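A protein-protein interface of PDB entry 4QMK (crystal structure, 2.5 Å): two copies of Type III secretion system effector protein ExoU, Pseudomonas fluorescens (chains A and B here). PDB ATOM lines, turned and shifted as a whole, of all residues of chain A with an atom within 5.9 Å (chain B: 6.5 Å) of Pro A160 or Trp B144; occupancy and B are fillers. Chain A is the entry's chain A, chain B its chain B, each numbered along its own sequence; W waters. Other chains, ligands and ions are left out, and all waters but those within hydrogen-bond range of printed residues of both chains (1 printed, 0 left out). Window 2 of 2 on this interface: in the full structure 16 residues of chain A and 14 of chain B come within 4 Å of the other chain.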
ATOM      1  N   LEU A 155      28.918 -20.334  32.128  1.00  0.00           N
ATOM      2  CA  LEU A 155      27.567 -20.798  31.980  1.00  0.00           C
ATOM      3  C   LEU A 155      26.659 -19.725  31.428  1.00  0.00           C
ATOM      4  O   LEU A 155      26.087 -19.883  30.340  1.00  0.00           O
ATOM      5  CB  LEU A 155      27.055 -21.314  33.301  1.00  0.00           C
ATOM      6  CG  LEU A 155      27.614 -22.672  33.741  1.00  0.00           C
ATOM      7  CD1 LEU A 155      27.294 -22.883  35.207  1.00  0.00           C
ATOM      8  CD2 LEU A 155      27.055 -23.823  32.930  1.00  0.00           C
ATOM      9  N   SER A 158      27.205 -18.402  27.756  1.00  0.00           N
ATOM     10  CA  SER A 158      27.141 -19.441  26.722  1.00  0.00           C
ATOM     11  C   SER A 158      25.756 -20.001  26.417  1.00  0.00           C
ATOM     12  O   SER A 158      25.646 -20.924  25.638  1.00  0.00           O
ATOM     13  CB  SER A 158      27.956 -20.640  27.200  1.00  0.00           C
ATOM     14  OG  SER A 158      27.274 -21.309  28.258  1.00  0.00           O
ATOM     15  N   LEU A 159      24.718 -19.472  27.040  1.00  0.00           N
ATOM     16  CA  LEU A 159      23.383 -20.012  26.877  1.00  0.00           C
ATOM     17  C   LEU A 159      22.778 -19.897  25.417  1.00  0.00           C
ATOM     18  O   LEU A 159      22.834 -18.856  24.757  1.00  0.00           O
ATOM     19  CB  LEU A 159      22.462 -19.368  27.909  1.00  0.00           C
ATOM     20  CG  LEU A 159      22.901 -19.563  29.376  1.00  0.00           C
ATOM     21  CD1 LEU A 159      21.909 -18.907  30.292  1.00  0.00           C
ATOM     22  CD2 LEU A 159      23.006 -21.027  29.733  1.00  0.00           C
ATOM     23  N   PRO A 160      22.193 -20.995  24.921  1.00  0.00           N
ATOM     24  CA  PRO A 160      21.587 -20.928  23.596  1.00  0.00           C
ATOM     25  C   PRO A 160      20.567 -19.794  23.512  1.00  0.00           C
ATOM     26  O   PRO A 160      20.448 -19.133  22.485  1.00  0.00           O
ATOM     27  CB  PRO A 160      20.897 -22.278  23.453  1.00  0.00           C
ATOM     28  CG  PRO A 160      20.701 -22.787  24.861  1.00  0.00           C
ATOM     29  CD  PRO A 160      21.834 -22.223  25.657  1.00  0.00           C
ATOM     30  N   GLY A 161      19.858 -19.572  24.611  1.00  0.00           N
ATOM     31  CA  GLY A 161      18.888 -18.521  24.703  1.00  0.00           C
ATOM     32  C   GLY A 161      19.206 -17.654  25.910  1.00  0.00           C
ATOM     33  O   GLY A 161      19.155 -18.121  27.070  1.00  0.00           O
ATOM     34  N   PRO A 162      19.501 -16.378  25.644  1.00  0.00           N
ATOM     35  CA  PRO A 162      19.851 -15.453  26.658  1.00  0.00           C
ATOM     36  C   PRO A 162      18.825 -15.338  27.808  1.00  0.00           C
ATOM     37  O   PRO A 162      17.607 -15.358  27.586  1.00  0.00           O
ATOM     38  CB  PRO A 162      19.887 -14.159  25.919  1.00  0.00           C
ATOM     39  CG  PRO A 162      18.809 -14.294  24.857  1.00  0.00           C
ATOM     40  CD  PRO A 162      19.017 -15.706  24.411  1.00  0.00           C
ATOM     41  N   PHE A 636      33.654 -22.295  26.114  1.00  0.00           N
ATOM     42  CA  PHE A 636      33.114 -20.930  26.128  1.00  0.00           C
ATOM     43  C   PHE A 636      34.128 -19.792  26.343  1.00  0.00           C
ATOM     44  O   PHE A 636      33.981 -18.979  27.271  1.00  0.00           O
ATOM     45  CB  PHE A 636      31.946 -20.831  27.133  1.00  0.00           C
ATOM     46  CG  PHE A 636      30.956 -21.958  27.012  1.00  0.00           C
ATOM     47  CD1 PHE A 636      30.298 -22.192  25.801  1.00  0.00           C
ATOM     48  CD2 PHE A 636      30.689 -22.790  28.094  1.00  0.00           C
ATOM     49  CE1 PHE A 636      29.384 -23.238  25.684  1.00  0.00           C
ATOM     50  CE2 PHE A 636      29.780 -23.838  27.984  1.00  0.00           C
ATOM     51  CZ  PHE A 636      29.121 -24.059  26.780  1.00  0.00           C
ATOM     52  N   ALA A 646      22.848 -15.569  18.982  1.00  0.00           N
ATOM     53  CA  ALA A 646      21.757 -15.969  19.872  1.00  0.00           C
ATOM     54  C   ALA A 646      20.739 -14.857  20.199  1.00  0.00           C
ATOM     55  O   ALA A 646      19.610 -15.155  20.537  1.00  0.00           O
ATOM     56  CB  ALA A 646      22.333 -16.483  21.185  1.00  0.00           C
ATOM     57  N   ASP B 139      20.516 -30.131  17.535  1.00  0.00           N
ATOM     58  CA  ASP B 139      19.877 -28.903  18.001  1.00  0.00           C
ATOM     59  C   ASP B 139      20.701 -28.253  19.119  1.00  0.00           C
ATOM     60  O   ASP B 139      21.410 -28.927  19.873  1.00  0.00           O
ATOM     61  CB  ASP B 139      18.449 -29.162  18.482  1.00  0.00           C
ATOM     62  CG  ASP B 139      18.406 -29.722  19.884  1.00  0.00           C
ATOM     63  OD1 ASP B 139      18.796 -30.894  20.066  1.00  0.00           O
ATOM     64  OD2 ASP B 139      17.977 -28.993  20.801  1.00  0.00           O
ATOM     65  N   PRO B 140      20.580 -26.939  19.251  1.00  0.00           N
ATOM     66  CA  PRO B 140      21.455 -26.190  20.161  1.00  0.00           C
ATOM     67  C   PRO B 140      21.346 -26.544  21.661  1.00  0.00           C
ATOM     68  O   PRO B 140      22.376 -26.649  22.338  1.00  0.00           O
ATOM     69  CB  PRO B 140      21.063 -24.723  19.904  1.00  0.00           C
ATOM     70  CG  PRO B 140      20.254 -24.728  18.650  1.00  0.00           C
ATOM     71  CD  PRO B 140      19.605 -26.069  18.574  1.00  0.00           C
ATOM     72  N   VAL B 141      20.134 -26.717  22.182  1.00  0.00           N
ATOM     73  CA  VAL B 141      19.970 -27.057  23.595  1.00  0.00           C
ATOM     74  C   VAL B 141      20.682 -28.348  23.966  1.00  0.00           C
ATOM     75  O   VAL B 141      21.423 -28.399  24.943  1.00  0.00           O
ATOM     76  CB  VAL B 141      18.502 -27.151  23.983  1.00  0.00           C
ATOM     77  CG1 VAL B 141      18.342 -27.778  25.364  1.00  0.00           C
ATOM     78  CG2 VAL B 141      17.878 -25.765  23.941  1.00  0.00           C
ATOM     79  N   THR B 142      20.447 -29.384  23.197  1.00  0.00           N
ATOM     80  CA  THR B 142      21.131 -30.629  23.415  1.00  0.00           C
ATOM     81  C   THR B 142      22.623 -30.400  23.338  1.00  0.00           C
ATOM     82  O   THR B 142      23.356 -30.861  24.198  1.00  0.00           O
ATOM     83  CB  THR B 142      20.767 -31.663  22.333  1.00  0.00           C
ATOM     84  OG1 THR B 142      19.359 -31.928  22.387  1.00  0.00           O
ATOM     85  CG2 THR B 142      21.560 -32.987  22.517  1.00  0.00           C
ATOM     86  N   ALA B 143      23.067 -29.697  22.303  1.00  0.00           N
ATOM     87  CA  ALA B 143      24.484 -29.439  22.119  1.00  0.00           C
ATOM     88  C   ALA B 143      25.079 -28.773  23.352  1.00  0.00           C
ATOM     89  O   ALA B 143      26.109 -29.186  23.857  1.00  0.00           O
ATOM     90  CB  ALA B 143      24.719 -28.567  20.893  1.00  0.00           C
ATOM     91  N   TRP B 144      24.413 -27.738  23.827  1.00  0.00           N
ATOM     92  CA  TRP B 144      24.857 -27.032  25.005  1.00  0.00           C
ATOM     93  C   TRP B 144      25.012 -27.984  26.191  1.00  0.00           C
ATOM     94  O   TRP B 144      25.942 -27.859  26.969  1.00  0.00           O
ATOM     95  CB  TRP B 144      23.861 -25.919  25.360  1.00  0.00           C
ATOM     96  CG  TRP B 144      24.250 -25.150  26.571  1.00  0.00           C
ATOM     97  CD1 TRP B 144      25.089 -24.132  26.622  1.00  0.00           C
ATOM     98  CD2 TRP B 144      23.818 -25.398  27.919  1.00  0.00           C
ATOM     99  NE1 TRP B 144      25.227 -23.691  27.924  1.00  0.00           N
ATOM    100  CE2 TRP B 144      24.450 -24.469  28.734  1.00  0.00           C
ATOM    101  CE3 TRP B 144      22.965 -26.327  28.501  1.00  0.00           C
ATOM    102  CZ2 TRP B 144      24.257 -24.419  30.117  1.00  0.00           C
ATOM    103  CZ3 TRP B 144      22.753 -26.272  29.891  1.00  0.00           C
ATOM    104  CH2 TRP B 144      23.413 -25.326  30.675  1.00  0.00           C
ATOM    105  N   LEU B 145      24.098 -28.923  26.345  1.00  0.00           N
ATOM    106  CA  LEU B 145      24.197 -29.863  27.430  1.00  0.00           C
ATOM    107  C   LEU B 145      25.453 -30.703  27.390  1.00  0.00           C
ATOM    108  O   LEU B 145      25.988 -30.978  28.432  1.00  0.00           O
ATOM    109  CB  LEU B 145      22.964 -30.744  27.516  1.00  0.00           C
ATOM    110  CG  LEU B 145      21.822 -30.038  28.218  1.00  0.00           C
ATOM    111  CD1 LEU B 145      20.496 -30.649  27.830  1.00  0.00           C
ATOM    112  CD2 LEU B 145      22.018 -30.090  29.727  1.00  0.00           C
ATOM    113  N   GLN B 146      25.923 -31.143  26.218  1.00  0.00           N
ATOM    114  CA  GLN B 146      27.209 -31.863  26.191  1.00  0.00           C
ATOM    115  C   GLN B 146      28.354 -30.970  26.651  1.00  0.00           C
ATOM    116  O   GLN B 146      29.096 -31.340  27.562  1.00  0.00           O
ATOM    117  CB  GLN B 146      27.566 -32.463  24.826  1.00  0.00           C
ATOM    118  CG  GLN B 146      27.067 -33.889  24.586  1.00  0.00           C
ATOM    119  CD  GLN B 146      25.618 -33.951  24.153  1.00  0.00           C
ATOM    120  OE1 GLN B 146      25.119 -33.048  23.462  1.00  0.00           O
ATOM    121  NE2 GLN B 146      24.920 -35.024  24.558  1.00  0.00           N
ATOM    122  N   GLU B 147      28.476 -29.791  26.048  1.00  0.00           N
ATOM    123  CA  GLU B 147      29.603 -28.914  26.347  1.00  0.00           C
ATOM    124  C   GLU B 147      29.626 -28.436  27.790  1.00  0.00           C
ATOM    125  O   GLU B 147      30.668 -28.366  28.410  1.00  0.00           O
ATOM    126  CB  GLU B 147      29.651 -27.718  25.378  1.00  0.00           C
ATOM    127  CG  GLU B 147      30.148 -28.058  23.961  1.00  0.00           C
ATOM    128  CD  GLU B 147      29.042 -28.540  23.005  1.00  0.00           C
ATOM    129  OE1 GLU B 147      28.118 -27.747  22.719  1.00  0.00           O
ATOM    130  OE2 GLU B 147      29.097 -29.695  22.509  1.00  0.00           O
ATOM    131  N   ALA B 148      28.455 -28.146  28.333  1.00  0.00           N
ATOM    132  CA  ALA B 148      28.337 -27.515  29.633  1.00  0.00           C
ATOM    133  C   ALA B 148      28.266 -28.487  30.800  1.00  0.00           C
ATOM    134  O   ALA B 148      28.308 -28.052  31.944  1.00  0.00           O
ATOM    135  CB  ALA B 148      27.105 -26.612  29.634  1.00  0.00           C
ATOM    136  N   SER B 149      28.178 -29.793  30.533  1.00  0.00           N
ATOM    137  CA  SER B 149      27.982 -30.778  31.594  1.00  0.00           C
ATOM    138  C   SER B 149      29.009 -30.696  32.703  1.00  0.00           C
ATOM    139  O   SER B 149      28.656 -30.749  33.861  1.00  0.00           O
ATOM    140  CB  SER B 149      27.911 -32.195  31.051  1.00  0.00           C
ATOM    141  OG  SER B 149      29.193 -32.767  30.972  1.00  0.00           O
ATOM    142  N   LEU B 152      28.484 -27.594  34.843  1.00  0.00           N
ATOM    143  CA  LEU B 152      27.287 -27.764  35.660  1.00  0.00           C
ATOM    144  C   LEU B 152      27.508 -28.650  36.874  1.00  0.00           C
ATOM    145  O   LEU B 152      26.856 -28.485  37.881  1.00  0.00           O
ATOM    146  CB  LEU B 152      26.157 -28.356  34.820  1.00  0.00           C
ATOM    147  CG  LEU B 152      25.406 -27.328  34.004  1.00  0.00           C
ATOM    148  CD1 LEU B 152      24.469 -28.011  33.037  1.00  0.00           C
ATOM    149  CD2 LEU B 152      24.623 -26.430  34.937  1.00  0.00           C
ATOM    150  N   LEU B 170      18.692 -26.218  35.495  1.00  0.00           N
ATOM    151  CA  LEU B 170      18.428 -26.319  34.060  1.00  0.00           C
ATOM    152  C   LEU B 170      17.216 -25.515  33.661  1.00  0.00           C
ATOM    153  O   LEU B 170      17.212 -24.825  32.629  1.00  0.00           O
ATOM    154  CB  LEU B 170      18.260 -27.764  33.666  1.00  0.00           C
ATOM    155  CG  LEU B 170      19.495 -28.593  33.961  1.00  0.00           C
ATOM    156  CD1 LEU B 170      19.270 -30.033  33.622  1.00  0.00           C
ATOM    157  CD2 LEU B 170      20.670 -28.077  33.167  1.00  0.00           C
ATOM    158  N   LEU B 173      18.451 -22.025  33.457  1.00  0.00           N
ATOM    159  CA  LEU B 173      19.488 -21.837  32.387  1.00  0.00           C
ATOM    160  C   LEU B 173      18.968 -22.088  30.977  1.00  0.00           C
ATOM    161  O   LEU B 173      19.499 -21.575  30.021  1.00  0.00           O
ATOM    162  CB  LEU B 173      20.680 -22.753  32.593  1.00  0.00           C
ATOM    163  CG  LEU B 173      21.501 -22.430  33.803  1.00  0.00           C
ATOM    164  CD1 LEU B 173      22.675 -23.375  33.906  1.00  0.00           C
ATOM    165  CD2 LEU B 173      21.964 -20.990  33.736  1.00  0.00           C
ATOM    166  N   LEU B 174      17.942 -22.913  30.855  1.00  0.00           N
ATOM    167  CA  LEU B 174      17.416 -23.269  29.544  1.00  0.00           C
ATOM    168  C   LEU B 174      15.916 -22.993  29.419  1.00  0.00           C
ATOM    169  O   LEU B 174      15.147 -23.900  29.142  1.00  0.00           O
ATOM    170  CB  LEU B 174      17.672 -24.757  29.289  1.00  0.00           C
ATOM    171  CG  LEU B 174      19.117 -25.197  29.233  1.00  0.00           C
ATOM    172  CD1 LEU B 174      19.181 -26.701  29.031  1.00  0.00           C
ATOM    173  CD2 LEU B 174      19.845 -24.495  28.120  1.00  0.00           C
ATOM    174  N   GLN B 182      12.390 -25.987  18.525  1.00  0.00           N
ATOM    175  CA  GLN B 182      12.944 -27.011  17.632  1.00  0.00           C
ATOM    176  C   GLN B 182      11.945 -28.133  17.383  1.00  0.00           C
ATOM    177  O   GLN B 182      11.078 -28.370  18.202  1.00  0.00           O
ATOM    178  CB  GLN B 182      14.205 -27.592  18.238  1.00  0.00           C
ATOM    179  CG  GLN B 182      15.238 -26.542  18.581  1.00  0.00           C
ATOM    180  CD  GLN B 182      15.597 -26.665  20.032  1.00  0.00           C
ATOM    181  OE1 GLN B 182      15.039 -27.524  20.725  1.00  0.00           O
ATOM    182  NE2 GLN B 182      16.483 -25.801  20.519  1.00  0.00           N
ATOM    183  N   ARG B 272       9.988 -28.938  26.627  1.00  0.00           N
ATOM    184  CA  ARG B 272      11.386 -28.589  26.930  1.00  0.00           C
ATOM    185  C   ARG B 272      11.980 -29.604  27.931  1.00  0.00           C
ATOM    186  O   ARG B 272      13.097 -30.098  27.728  1.00  0.00           O
ATOM    187  CB  ARG B 272      11.438 -27.135  27.438  1.00  0.00           C
ATOM    188  CG  ARG B 272      12.787 -26.567  27.866  1.00  0.00           C
ATOM    189  CD  ARG B 272      13.931 -26.863  26.901  1.00  0.00           C
ATOM    190  NE  ARG B 272      13.785 -26.240  25.575  1.00  0.00           N
ATOM    191  CZ  ARG B 272      14.218 -25.027  25.254  1.00  0.00           C
ATOM    192  NH1 ARG B 272      14.806 -24.258  26.147  1.00  0.00           N
ATOM    193  NH2 ARG B 272      14.035 -24.574  24.039  1.00  0.00           N
HETATM  194  O   HOH W   1      18.844 -20.726  27.545  1.00  0.00           O
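The side-chain hydroxyl (OG) of Ser A158 lies within hydrogen-bond range of the indole nitrogen (NE1) of Trp B144.
The guanidinium group (NH1) of Arg B272 is in hydrogen-bond range of the backbone carbonyl oxygen (O) of Leu B174 (3.0 Å). OE1 of Glu B147 sits close to O of Ala B143 (2.7 Å). The backbone carbonyl oxygen (O) of Leu A155 is in hydrogen-bond range of the side-chain hydroxyl (OG) of Ser A158 (2.8 Å).
Leu A159 touches Trp B144 (CD2 to CZ2, 3.6 Å). Leu B173 touches Leu A159. Pro A160 touches Trp B144. CG of Pro A160 touches CD2 of Leu B174, at 3.8 Å. Phe A636 touches Glu B147 (CZ to CB, 3.95 Å).
Pro A160 touches just these residues of chain B: Trp B144 (3.9 Å) and Leu B174 (3.8 Å). Printed residues of chain A within 4 Å of Trp B144: Ser A158 (3.2 Å), Leu A159 (3.6 Å) and Pro A160 (3.9 Å). Of the printed residues of chain B, Leu A159 touches Trp B144 and Leu B173. Printed residues of chain A within 4 Å of Glu B147: Phe A636. The nearest printed residue of chain A that does not touch Trp B144 is Leu A155 (4.01 Å). The nearest printed residue of chain B that does not touch Ser A158 is Ala B148 (5.5 Å).
Of the 17 printed residues of chain B, 4 touch a printed residue of chain A. Hydrophobic or aromatic side chains of chain B within 4 Å of the printed part of chain A: Trp B144 and Leu B174. Printed residues of chain A that touch a printed residue of chain B: Ser A158, Leu A159, Pro A160 and Phe A636. Hydrophobic or aromatic side chains of chain A within 4 Å of the printed part of chain B: Leu A159, Pro A160 and Phe A636. Among the printed residues, 6 pairs touch across the chains.
No position is printed for both chains.
Water W1 lies within hydrogen-bond range of the backbone carbonyl oxygen of Gly A161 (2.7 Å) and the backbone carbonyl oxygen of Leu B173 (2.7 Å).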
